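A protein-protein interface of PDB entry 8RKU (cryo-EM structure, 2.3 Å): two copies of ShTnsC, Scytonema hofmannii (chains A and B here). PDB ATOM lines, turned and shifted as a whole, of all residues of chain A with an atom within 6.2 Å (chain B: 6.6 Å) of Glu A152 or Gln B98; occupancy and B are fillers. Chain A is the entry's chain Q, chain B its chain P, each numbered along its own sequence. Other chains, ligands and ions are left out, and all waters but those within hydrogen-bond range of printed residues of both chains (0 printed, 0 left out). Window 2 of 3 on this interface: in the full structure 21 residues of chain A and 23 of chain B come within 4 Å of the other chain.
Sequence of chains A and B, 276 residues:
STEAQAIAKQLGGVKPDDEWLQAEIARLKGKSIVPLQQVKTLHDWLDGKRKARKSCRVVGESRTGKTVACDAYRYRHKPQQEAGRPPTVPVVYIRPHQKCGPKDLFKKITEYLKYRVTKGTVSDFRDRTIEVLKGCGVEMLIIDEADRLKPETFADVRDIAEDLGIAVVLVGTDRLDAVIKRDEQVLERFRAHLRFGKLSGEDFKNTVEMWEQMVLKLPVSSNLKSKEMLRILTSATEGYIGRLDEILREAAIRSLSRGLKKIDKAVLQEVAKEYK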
ATOM      1  N   CYS A 100      14.774   0.215   1.729  1.00  0.00           N
ATOM      2  CA  CYS A 100      14.273  -0.687   0.701  1.00  0.00           C
ATOM      3  C   CYS A 100      15.012  -2.022   0.751  1.00  0.00           C
ATOM      4  O   CYS A 100      16.232  -2.069   0.568  1.00  0.00           O
ATOM      5  CB  CYS A 100      14.426  -0.045  -0.673  1.00  0.00           C
ATOM      6  SG  CYS A 100      13.668  -0.977  -2.016  1.00  0.00           S
ATOM      7  N   GLY A 101      14.278  -3.102   0.997  1.00  0.00           N
ATOM      8  CA  GLY A 101      14.827  -4.430   0.843  1.00  0.00           C
ATOM      9  C   GLY A 101      14.787  -4.888  -0.595  1.00  0.00           C
ATOM     10  O   GLY A 101      14.202  -4.247  -1.477  1.00  0.00           O
ATOM     11  N   PRO A 102      15.444  -6.023  -0.859  1.00  0.00           N
ATOM     12  CA  PRO A 102      15.409  -6.576  -2.224  1.00  0.00           C
ATOM     13  C   PRO A 102      14.006  -6.823  -2.744  1.00  0.00           C
ATOM     14  O   PRO A 102      13.721  -6.518  -3.907  1.00  0.00           O
ATOM     15  CB  PRO A 102      16.206  -7.881  -2.087  1.00  0.00           C
ATOM     16  CG  PRO A 102      17.111  -7.641  -0.933  1.00  0.00           C
ATOM     17  CD  PRO A 102      16.310  -6.809   0.028  1.00  0.00           C
ATOM     18  N   ARG A 126      13.146 -12.102  -7.361  1.00  0.00           N
ATOM     19  CA  ARG A 126      14.358 -11.918  -8.154  1.00  0.00           C
ATOM     20  C   ARG A 126      14.217 -12.466  -9.573  1.00  0.00           C
ATOM     21  O   ARG A 126      14.466 -11.751 -10.548  1.00  0.00           O
ATOM     22  CB  ARG A 126      15.541 -12.562  -7.437  1.00  0.00           C
ATOM     23  CG  ARG A 126      16.887 -12.292  -8.072  1.00  0.00           C
ATOM     24  CD  ARG A 126      17.991 -12.943  -7.267  1.00  0.00           C
ATOM     25  NE  ARG A 126      18.146 -12.305  -5.967  1.00  0.00           N
ATOM     26  CZ  ARG A 126      17.808 -12.864  -4.815  1.00  0.00           C
ATOM     27  NH1 ARG A 126      17.387 -14.115  -4.753  1.00  0.00           N
ATOM     28  NH2 ARG A 126      17.918 -12.156  -3.693  1.00  0.00           N
ATOM     29  N   LYS A 150      18.965  -0.594   1.560  1.00  0.00           N
ATOM     30  CA  LYS A 150      19.688  -1.309   2.603  1.00  0.00           C
ATOM     31  C   LYS A 150      20.980  -1.931   2.065  1.00  0.00           C
ATOM     32  O   LYS A 150      21.081  -2.254   0.879  1.00  0.00           O
ATOM     33  CB  LYS A 150      18.801  -2.389   3.220  1.00  0.00           C
ATOM     34  CG  LYS A 150      17.625  -1.818   3.995  1.00  0.00           C
ATOM     35  CD  LYS A 150      16.930  -2.869   4.838  1.00  0.00           C
ATOM     36  CE  LYS A 150      16.131  -3.828   3.997  1.00  0.00           C
ATOM     37  NZ  LYS A 150      15.949  -5.139   4.674  1.00  0.00           N
ATOM     38  N   PRO A 151      21.990  -2.098   2.931  1.00  0.00           N
ATOM     39  CA  PRO A 151      23.283  -2.662   2.493  1.00  0.00           C
ATOM     40  C   PRO A 151      23.240  -4.008   1.769  1.00  0.00           C
ATOM     41  O   PRO A 151      24.049  -4.219   0.856  1.00  0.00           O
ATOM     42  CB  PRO A 151      24.064  -2.777   3.811  1.00  0.00           C
ATOM     43  CG  PRO A 151      23.493  -1.722   4.682  1.00  0.00           C
ATOM     44  CD  PRO A 151      22.032  -1.656   4.337  1.00  0.00           C
ATOM     45  N   GLU A 152      22.349  -4.930   2.145  1.00  0.00           N
ATOM     46  CA  GLU A 152      22.243  -6.183   1.396  1.00  0.00           C
ATOM     47  C   GLU A 152      21.612  -5.985   0.023  1.00  0.00           C
ATOM     48  O   GLU A 152      21.896  -6.755  -0.902  1.00  0.00           O
ATOM     49  CB  GLU A 152      21.467  -7.233   2.195  1.00  0.00           C
ATOM     50  CG  GLU A 152      19.960  -7.049   2.240  1.00  0.00           C
ATOM     51  CD  GLU A 152      19.512  -6.096   3.324  1.00  0.00           C
ATOM     52  OE1 GLU A 152      20.337  -5.279   3.784  1.00  0.00           O
ATOM     53  OE2 GLU A 152      18.332  -6.175   3.722  1.00  0.00           O
ATOM     54  N   THR A 153      20.759  -4.970  -0.132  1.00  0.00           N
ATOM     55  CA  THR A 153      20.082  -4.751  -1.408  1.00  0.00           C
ATOM     56  C   THR A 153      21.061  -4.331  -2.501  1.00  0.00           C
ATOM     57  O   THR A 153      20.834  -4.620  -3.680  1.00  0.00           O
ATOM     58  CB  THR A 153      18.980  -3.704  -1.231  1.00  0.00           C
ATOM     59  OG1 THR A 153      18.160  -4.068  -0.115  1.00  0.00           O
ATOM     60  CG2 THR A 153      18.105  -3.629  -2.465  1.00  0.00           C
ATOM     61  N   PHE A 154      22.150  -3.656  -2.126  1.00  0.00           N
ATOM     62  CA  PHE A 154      23.210  -3.312  -3.073  1.00  0.00           C
ATOM     63  C   PHE A 154      23.831  -4.532  -3.740  1.00  0.00           C
ATOM     64  O   PHE A 154      24.370  -4.420  -4.846  1.00  0.00           O
ATOM     65  CB  PHE A 154      24.290  -2.490  -2.373  1.00  0.00           C
ATOM     66  CG  PHE A 154      23.917  -1.056  -2.181  1.00  0.00           C
ATOM     67  CD1 PHE A 154      24.131  -0.133  -3.190  1.00  0.00           C
ATOM     68  CD2 PHE A 154      23.342  -0.628  -1.001  1.00  0.00           C
ATOM     69  CE1 PHE A 154      23.790   1.188  -3.021  1.00  0.00           C
ATOM     70  CE2 PHE A 154      22.998   0.692  -0.825  1.00  0.00           C
ATOM     71  CZ  PHE A 154      23.221   1.601  -1.837  1.00  0.00           C
ATOM     72  N   ALA A 155      23.786  -5.696  -3.093  1.00  0.00           N
ATOM     73  CA  ALA A 155      24.278  -6.907  -3.742  1.00  0.00           C
ATOM     74  C   ALA A 155      23.387  -7.323  -4.905  1.00  0.00           C
ATOM     75  O   ALA A 155      23.885  -7.785  -5.937  1.00  0.00           O
ATOM     76  CB  ALA A 155      24.388  -8.042  -2.724  1.00  0.00           C
ATOM     77  N   ASP A 156      22.071  -7.172  -4.765  1.00  0.00           N
ATOM     78  CA  ASP A 156      21.186  -7.383  -5.905  1.00  0.00           C
ATOM     79  C   ASP A 156      21.347  -6.288  -6.954  1.00  0.00           C
ATOM     80  O   ASP A 156      21.348  -6.567  -8.158  1.00  0.00           O
ATOM     81  CB  ASP A 156      19.734  -7.461  -5.437  1.00  0.00           C
ATOM     82  CG  ASP A 156      19.370  -8.819  -4.874  1.00  0.00           C
ATOM     83  OD1 ASP A 156      19.626  -9.835  -5.551  1.00  0.00           O
ATOM     84  OD2 ASP A 156      18.820  -8.871  -3.757  1.00  0.00           O
ATOM     85  N   VAL A 157      21.495  -5.037  -6.514  1.00  0.00           N
ATOM     86  CA  VAL A 157      21.736  -3.925  -7.432  1.00  0.00           C
ATOM     87  C   VAL A 157      23.023  -4.113  -8.226  1.00  0.00           C
ATOM     88  O   VAL A 157      23.061  -3.863  -9.437  1.00  0.00           O
ATOM     89  CB  VAL A 157      21.750  -2.599  -6.647  1.00  0.00           C
ATOM     90  CG1 VAL A 157      22.206  -1.460  -7.531  1.00  0.00           C
ATOM     91  CG2 VAL A 157      20.376  -2.314  -6.073  1.00  0.00           C
ATOM     92  N   ASP A 159      24.463  -7.054  -8.909  1.00  0.00           N
ATOM     93  CA  ASP A 159      24.292  -8.176  -9.827  1.00  0.00           C
ATOM     94  C   ASP A 159      23.364  -7.843 -10.988  1.00  0.00           C
ATOM     95  O   ASP A 159      23.604  -8.278 -12.118  1.00  0.00           O
ATOM     96  CB  ASP A 159      23.787  -9.392  -9.055  1.00  0.00           C
ATOM     97  CG  ASP A 159      24.872 -10.027  -8.212  1.00  0.00           C
ATOM     98  OD1 ASP A 159      25.907  -9.364  -7.989  1.00  0.00           O
ATOM     99  OD2 ASP A 159      24.696 -11.183  -7.772  1.00  0.00           O
ATOM    100  N   PRO B  96      26.708 -17.267  -4.965  1.00  0.00           N
ATOM    101  CA  PRO B  96      25.478 -17.168  -4.181  1.00  0.00           C
ATOM    102  C   PRO B  96      24.779 -15.837  -4.382  1.00  0.00           C
ATOM    103  O   PRO B  96      25.407 -14.807  -4.628  1.00  0.00           O
ATOM    104  CB  PRO B  96      25.966 -17.325  -2.736  1.00  0.00           C
ATOM    105  CG  PRO B  96      27.258 -18.008  -2.851  1.00  0.00           C
ATOM    106  CD  PRO B  96      27.874 -17.500  -4.107  1.00  0.00           C
ATOM    107  N   HIS B  97      23.457 -15.873  -4.289  1.00  0.00           N
ATOM    108  CA  HIS B  97      22.694 -14.665  -4.041  1.00  0.00           C
ATOM    109  C   HIS B  97      22.931 -14.196  -2.609  1.00  0.00           C
ATOM    110  O   HIS B  97      23.381 -14.952  -1.748  1.00  0.00           O
ATOM    111  CB  HIS B  97      21.210 -14.905  -4.310  1.00  0.00           C
ATOM    112  CG  HIS B  97      20.929 -15.399  -5.694  1.00  0.00           C
ATOM    113  ND1 HIS B  97      21.220 -14.663  -6.820  1.00  0.00           N
ATOM    114  CD2 HIS B  97      20.398 -16.565  -6.134  1.00  0.00           C
ATOM    115  CE1 HIS B  97      20.874 -15.347  -7.895  1.00  0.00           C
ATOM    116  NE2 HIS B  97      20.371 -16.504  -7.506  1.00  0.00           N
ATOM    117  N   GLN B  98      22.645 -12.923  -2.366  1.00  0.00           N
ATOM    118  CA  GLN B  98      22.861 -12.357  -1.042  1.00  0.00           C
ATOM    119  C   GLN B  98      22.002 -13.079  -0.006  1.00  0.00           C
ATOM    120  O   GLN B  98      20.877 -13.501  -0.285  1.00  0.00           O
ATOM    121  CB  GLN B  98      22.527 -10.864  -1.052  1.00  0.00           C
ATOM    122  CG  GLN B  98      22.787 -10.096   0.244  1.00  0.00           C
ATOM    123  CD  GLN B  98      24.222 -10.189   0.734  1.00  0.00           C
ATOM    124  OE1 GLN B  98      24.696 -11.250   1.138  1.00  0.00           O
ATOM    125  NE2 GLN B  98      24.924  -9.064   0.696  1.00  0.00           N
ATOM    126  N   LYS B  99      22.548 -13.212   1.203  1.00  0.00           N
ATOM    127  CA  LYS B  99      21.963 -14.022   2.277  1.00  0.00           C
ATOM    128  C   LYS B  99      21.607 -15.427   1.795  1.00  0.00           C
ATOM    129  O   LYS B  99      20.479 -15.897   1.951  1.00  0.00           O
ATOM    130  CB  LYS B  99      20.739 -13.329   2.880  1.00  0.00           C
ATOM    131  CG  LYS B  99      21.036 -11.988   3.526  1.00  0.00           C
ATOM    132  CD  LYS B  99      22.095 -12.131   4.604  1.00  0.00           C
ATOM    133  CE  LYS B  99      22.331 -10.820   5.338  1.00  0.00           C
ATOM    134  NZ  LYS B  99      21.210 -10.477   6.256  1.00  0.00           N
ATOM    135  N   CYS B 100      22.588 -16.099   1.199  1.00  0.00           N
ATOM    136  CA  CYS B 100      22.398 -17.462   0.716  1.00  0.00           C
ATOM    137  C   CYS B 100      22.264 -18.419   1.894  1.00  0.00           C
ATOM    138  O   CYS B 100      23.215 -18.609   2.656  1.00  0.00           O
ATOM    139  CB  CYS B 100      23.564 -17.867  -0.179  1.00  0.00           C
ATOM    140  SG  CYS B 100      23.499 -19.564  -0.794  1.00  0.00           S
ATOM    141  N   GLY B 101      21.095 -19.035   2.036  1.00  0.00           N
ATOM    142  CA  GLY B 101      20.925 -20.114   2.976  1.00  0.00           C
ATOM    143  C   GLY B 101      21.323 -21.465   2.419  1.00  0.00           C
ATOM    144  O   GLY B 101      21.770 -21.585   1.276  1.00  0.00           O
ATOM    145  N   ASP B 104      19.358 -22.398  -0.764  1.00  0.00           N
ATOM    146  CA  ASP B 104      19.855 -21.624  -1.896  1.00  0.00           C
ATOM    147  C   ASP B 104      21.170 -22.176  -2.430  1.00  0.00           C
ATOM    148  O   ASP B 104      21.369 -22.255  -3.647  1.00  0.00           O
ATOM    149  CB  ASP B 104      20.028 -20.165  -1.480  1.00  0.00           C
ATOM    150  CG  ASP B 104      18.766 -19.576  -0.889  1.00  0.00           C
ATOM    151  OD1 ASP B 104      17.669 -20.082  -1.205  1.00  0.00           O
ATOM    152  OD2 ASP B 104      18.866 -18.615  -0.097  1.00  0.00           O
ATOM    153  N   ASP B 147      31.445 -14.452   0.900  1.00  0.00           N
ATOM    154  CA  ASP B 147      30.929 -13.680   2.027  1.00  0.00           C
ATOM    155  C   ASP B 147      29.413 -13.513   2.010  1.00  0.00           C
ATOM    156  O   ASP B 147      28.850 -13.059   3.009  1.00  0.00           O
ATOM    157  CB  ASP B 147      31.592 -12.306   2.071  1.00  0.00           C
ATOM    158  CG  ASP B 147      31.412 -11.530   0.786  1.00  0.00           C
ATOM    159  OD1 ASP B 147      32.016 -11.922  -0.232  1.00  0.00           O
ATOM    160  OD2 ASP B 147      30.666 -10.528   0.791  1.00  0.00           O
ATOM    161  N   ARG B 148      28.743 -13.840   0.906  1.00  0.00           N
ATOM    162  CA  ARG B 148      27.286 -13.816   0.873  1.00  0.00           C
ATOM    163  C   ARG B 148      26.642 -15.008   1.571  1.00  0.00           C
ATOM    164  O   ARG B 148      25.444 -14.955   1.870  1.00  0.00           O
ATOM    165  CB  ARG B 148      26.806 -13.778  -0.575  1.00  0.00           C
ATOM    166  CG  ARG B 148      27.120 -12.502  -1.310  1.00  0.00           C
ATOM    167  CD  ARG B 148      26.550 -12.575  -2.698  1.00  0.00           C
ATOM    168  NE  ARG B 148      26.783 -11.364  -3.470  1.00  0.00           N
ATOM    169  CZ  ARG B 148      26.269 -11.144  -4.672  1.00  0.00           C
ATOM    170  NH1 ARG B 148      25.509 -12.042  -5.270  1.00  0.00           N
ATOM    171  NH2 ARG B 148      26.541 -10.000  -5.291  1.00  0.00           N
ATOM    172  N   LEU B 149      27.396 -16.074   1.830  1.00  0.00           N
ATOM    173  CA  LEU B 149      26.860 -17.218   2.559  1.00  0.00           C
ATOM    174  C   LEU B 149      26.458 -16.822   3.973  1.00  0.00           C
ATOM    175  O   LEU B 149      27.220 -16.166   4.688  1.00  0.00           O
ATOM    176  CB  LEU B 149      27.889 -18.346   2.591  1.00  0.00           C
ATOM    177  CG  LEU B 149      28.245 -18.916   1.226  1.00  0.00           C
ATOM    178  CD1 LEU B 149      29.313 -19.979   1.346  1.00  0.00           C
ATOM    179  CD2 LEU B 149      26.997 -19.474   0.590  1.00  0.00           C
ATOM    180  N   LYS B 150      25.249 -17.216   4.371  1.00  0.00           N
ATOM    181  CA  LYS B 150      24.833 -17.085   5.760  1.00  0.00           C
ATOM    182  C   LYS B 150      25.752 -17.873   6.696  1.00  0.00           C
ATOM    183  O   LYS B 150      26.281 -18.925   6.327  1.00  0.00           O
ATOM    184  CB  LYS B 150      23.399 -17.576   5.937  1.00  0.00           C
ATOM    185  CG  LYS B 150      22.329 -16.659   5.393  1.00  0.00           C
ATOM    186  CD  LYS B 150      20.954 -17.177   5.783  1.00  0.00           C
ATOM    187  CE  LYS B 150      19.842 -16.311   5.228  1.00  0.00           C
ATOM    188  NZ  LYS B 150      18.503 -16.806   5.654  1.00  0.00           N
ATOM    189  N   ARG B 175      36.521  -8.343   3.017  1.00  0.00           N
ATOM    190  CA  ARG B 175      35.218  -8.502   3.656  1.00  0.00           C
ATOM    191  C   ARG B 175      34.926  -9.959   3.997  1.00  0.00           C
ATOM    192  O   ARG B 175      34.238 -10.242   4.984  1.00  0.00           O
ATOM    193  CB  ARG B 175      34.141  -7.923   2.737  1.00  0.00           C
ATOM    194  CG  ARG B 175      32.824  -7.543   3.394  1.00  0.00           C
ATOM    195  CD  ARG B 175      31.705  -7.594   2.367  1.00  0.00           C
ATOM    196  NE  ARG B 175      30.744  -6.505   2.512  1.00  0.00           N
ATOM    197  CZ  ARG B 175      29.855  -6.390   3.489  1.00  0.00           C
ATOM    198  NH1 ARG B 175      29.821  -7.240   4.503  1.00  0.00           N
ATOM    199  NH2 ARG B 175      28.998  -5.372   3.468  1.00  0.00           N
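Glu A152 touches one residue of chain B. Printed residues of chain B within 4 Å of Ala A155: Gln B98 and Arg B148. Printed residues of chain A within 4 Å of His B97: Arg A126 (3.7 Å). Gln B98 touches two residues of chain A. Of the printed residues of chain A, Arg B148 touches Ala A155 (3.5 Å) and Asp A159 (2.8 Å). The nearest residue of chain B that does not touch Glu A152 is Lys B99 (4.8 Å). The nearest residue of chain A that does not touch Gln B98 is Arg A126 (4.7 Å). The nearest printed residue of chain A that does not touch Arg B148 is Asp A156 (5.3 Å).
3 positions are printed for both chains. Of the 5 pairs that touch across the chains among the printed residues, none has its exchanged pair printed and touching as well.
O of Pro B96 is in hydrogen-bond range of NH1 of Arg B148, 2.8 Å away. O of Arg B148 is in hydrogen-bond range of N of Lys B99, 3.4 Å away. N of Cys B100 sits at hydrogen-bond distance from O of Arg B148 (3.1 Å). The guanidinium group (NE) of Arg A126 is in salt-bridge range of the side-chain carboxylate (OD1) of Asp A156 (2.9 Å). The side-chain carboxylate of Glu A152 lies within salt-bridge range of the side-chain amino group of Lys A150, at 2.8 Å.
Among the printed residues, merely in contact across the chains: Arg A126 with His B97, Glu A152 with Gln B98, Ala A155 with Gln B98 and Ala A155 with Arg B148.
The guanidinium group of Arg B148 is in salt-bridge range of the side-chain carboxylate of Asp A159 (2.8 Å).
Hydrophobic or aromatic side chains of chain A that line the printed part of chain B: Ala A155. Of the 12 printed residues of chain B, 3 touch a printed residue of chain A. Printed residues of chain B that touch a printed residue of chain A: His B97, Gln B98 and Arg B148. Among the printed residues, 5 pairs touch across the chains. Among the printed residues, Asp or Glu carboxylates within 4 Å of a Lys or Arg side-chain nitrogen of the other chain: Asp A159 with Arg B148.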
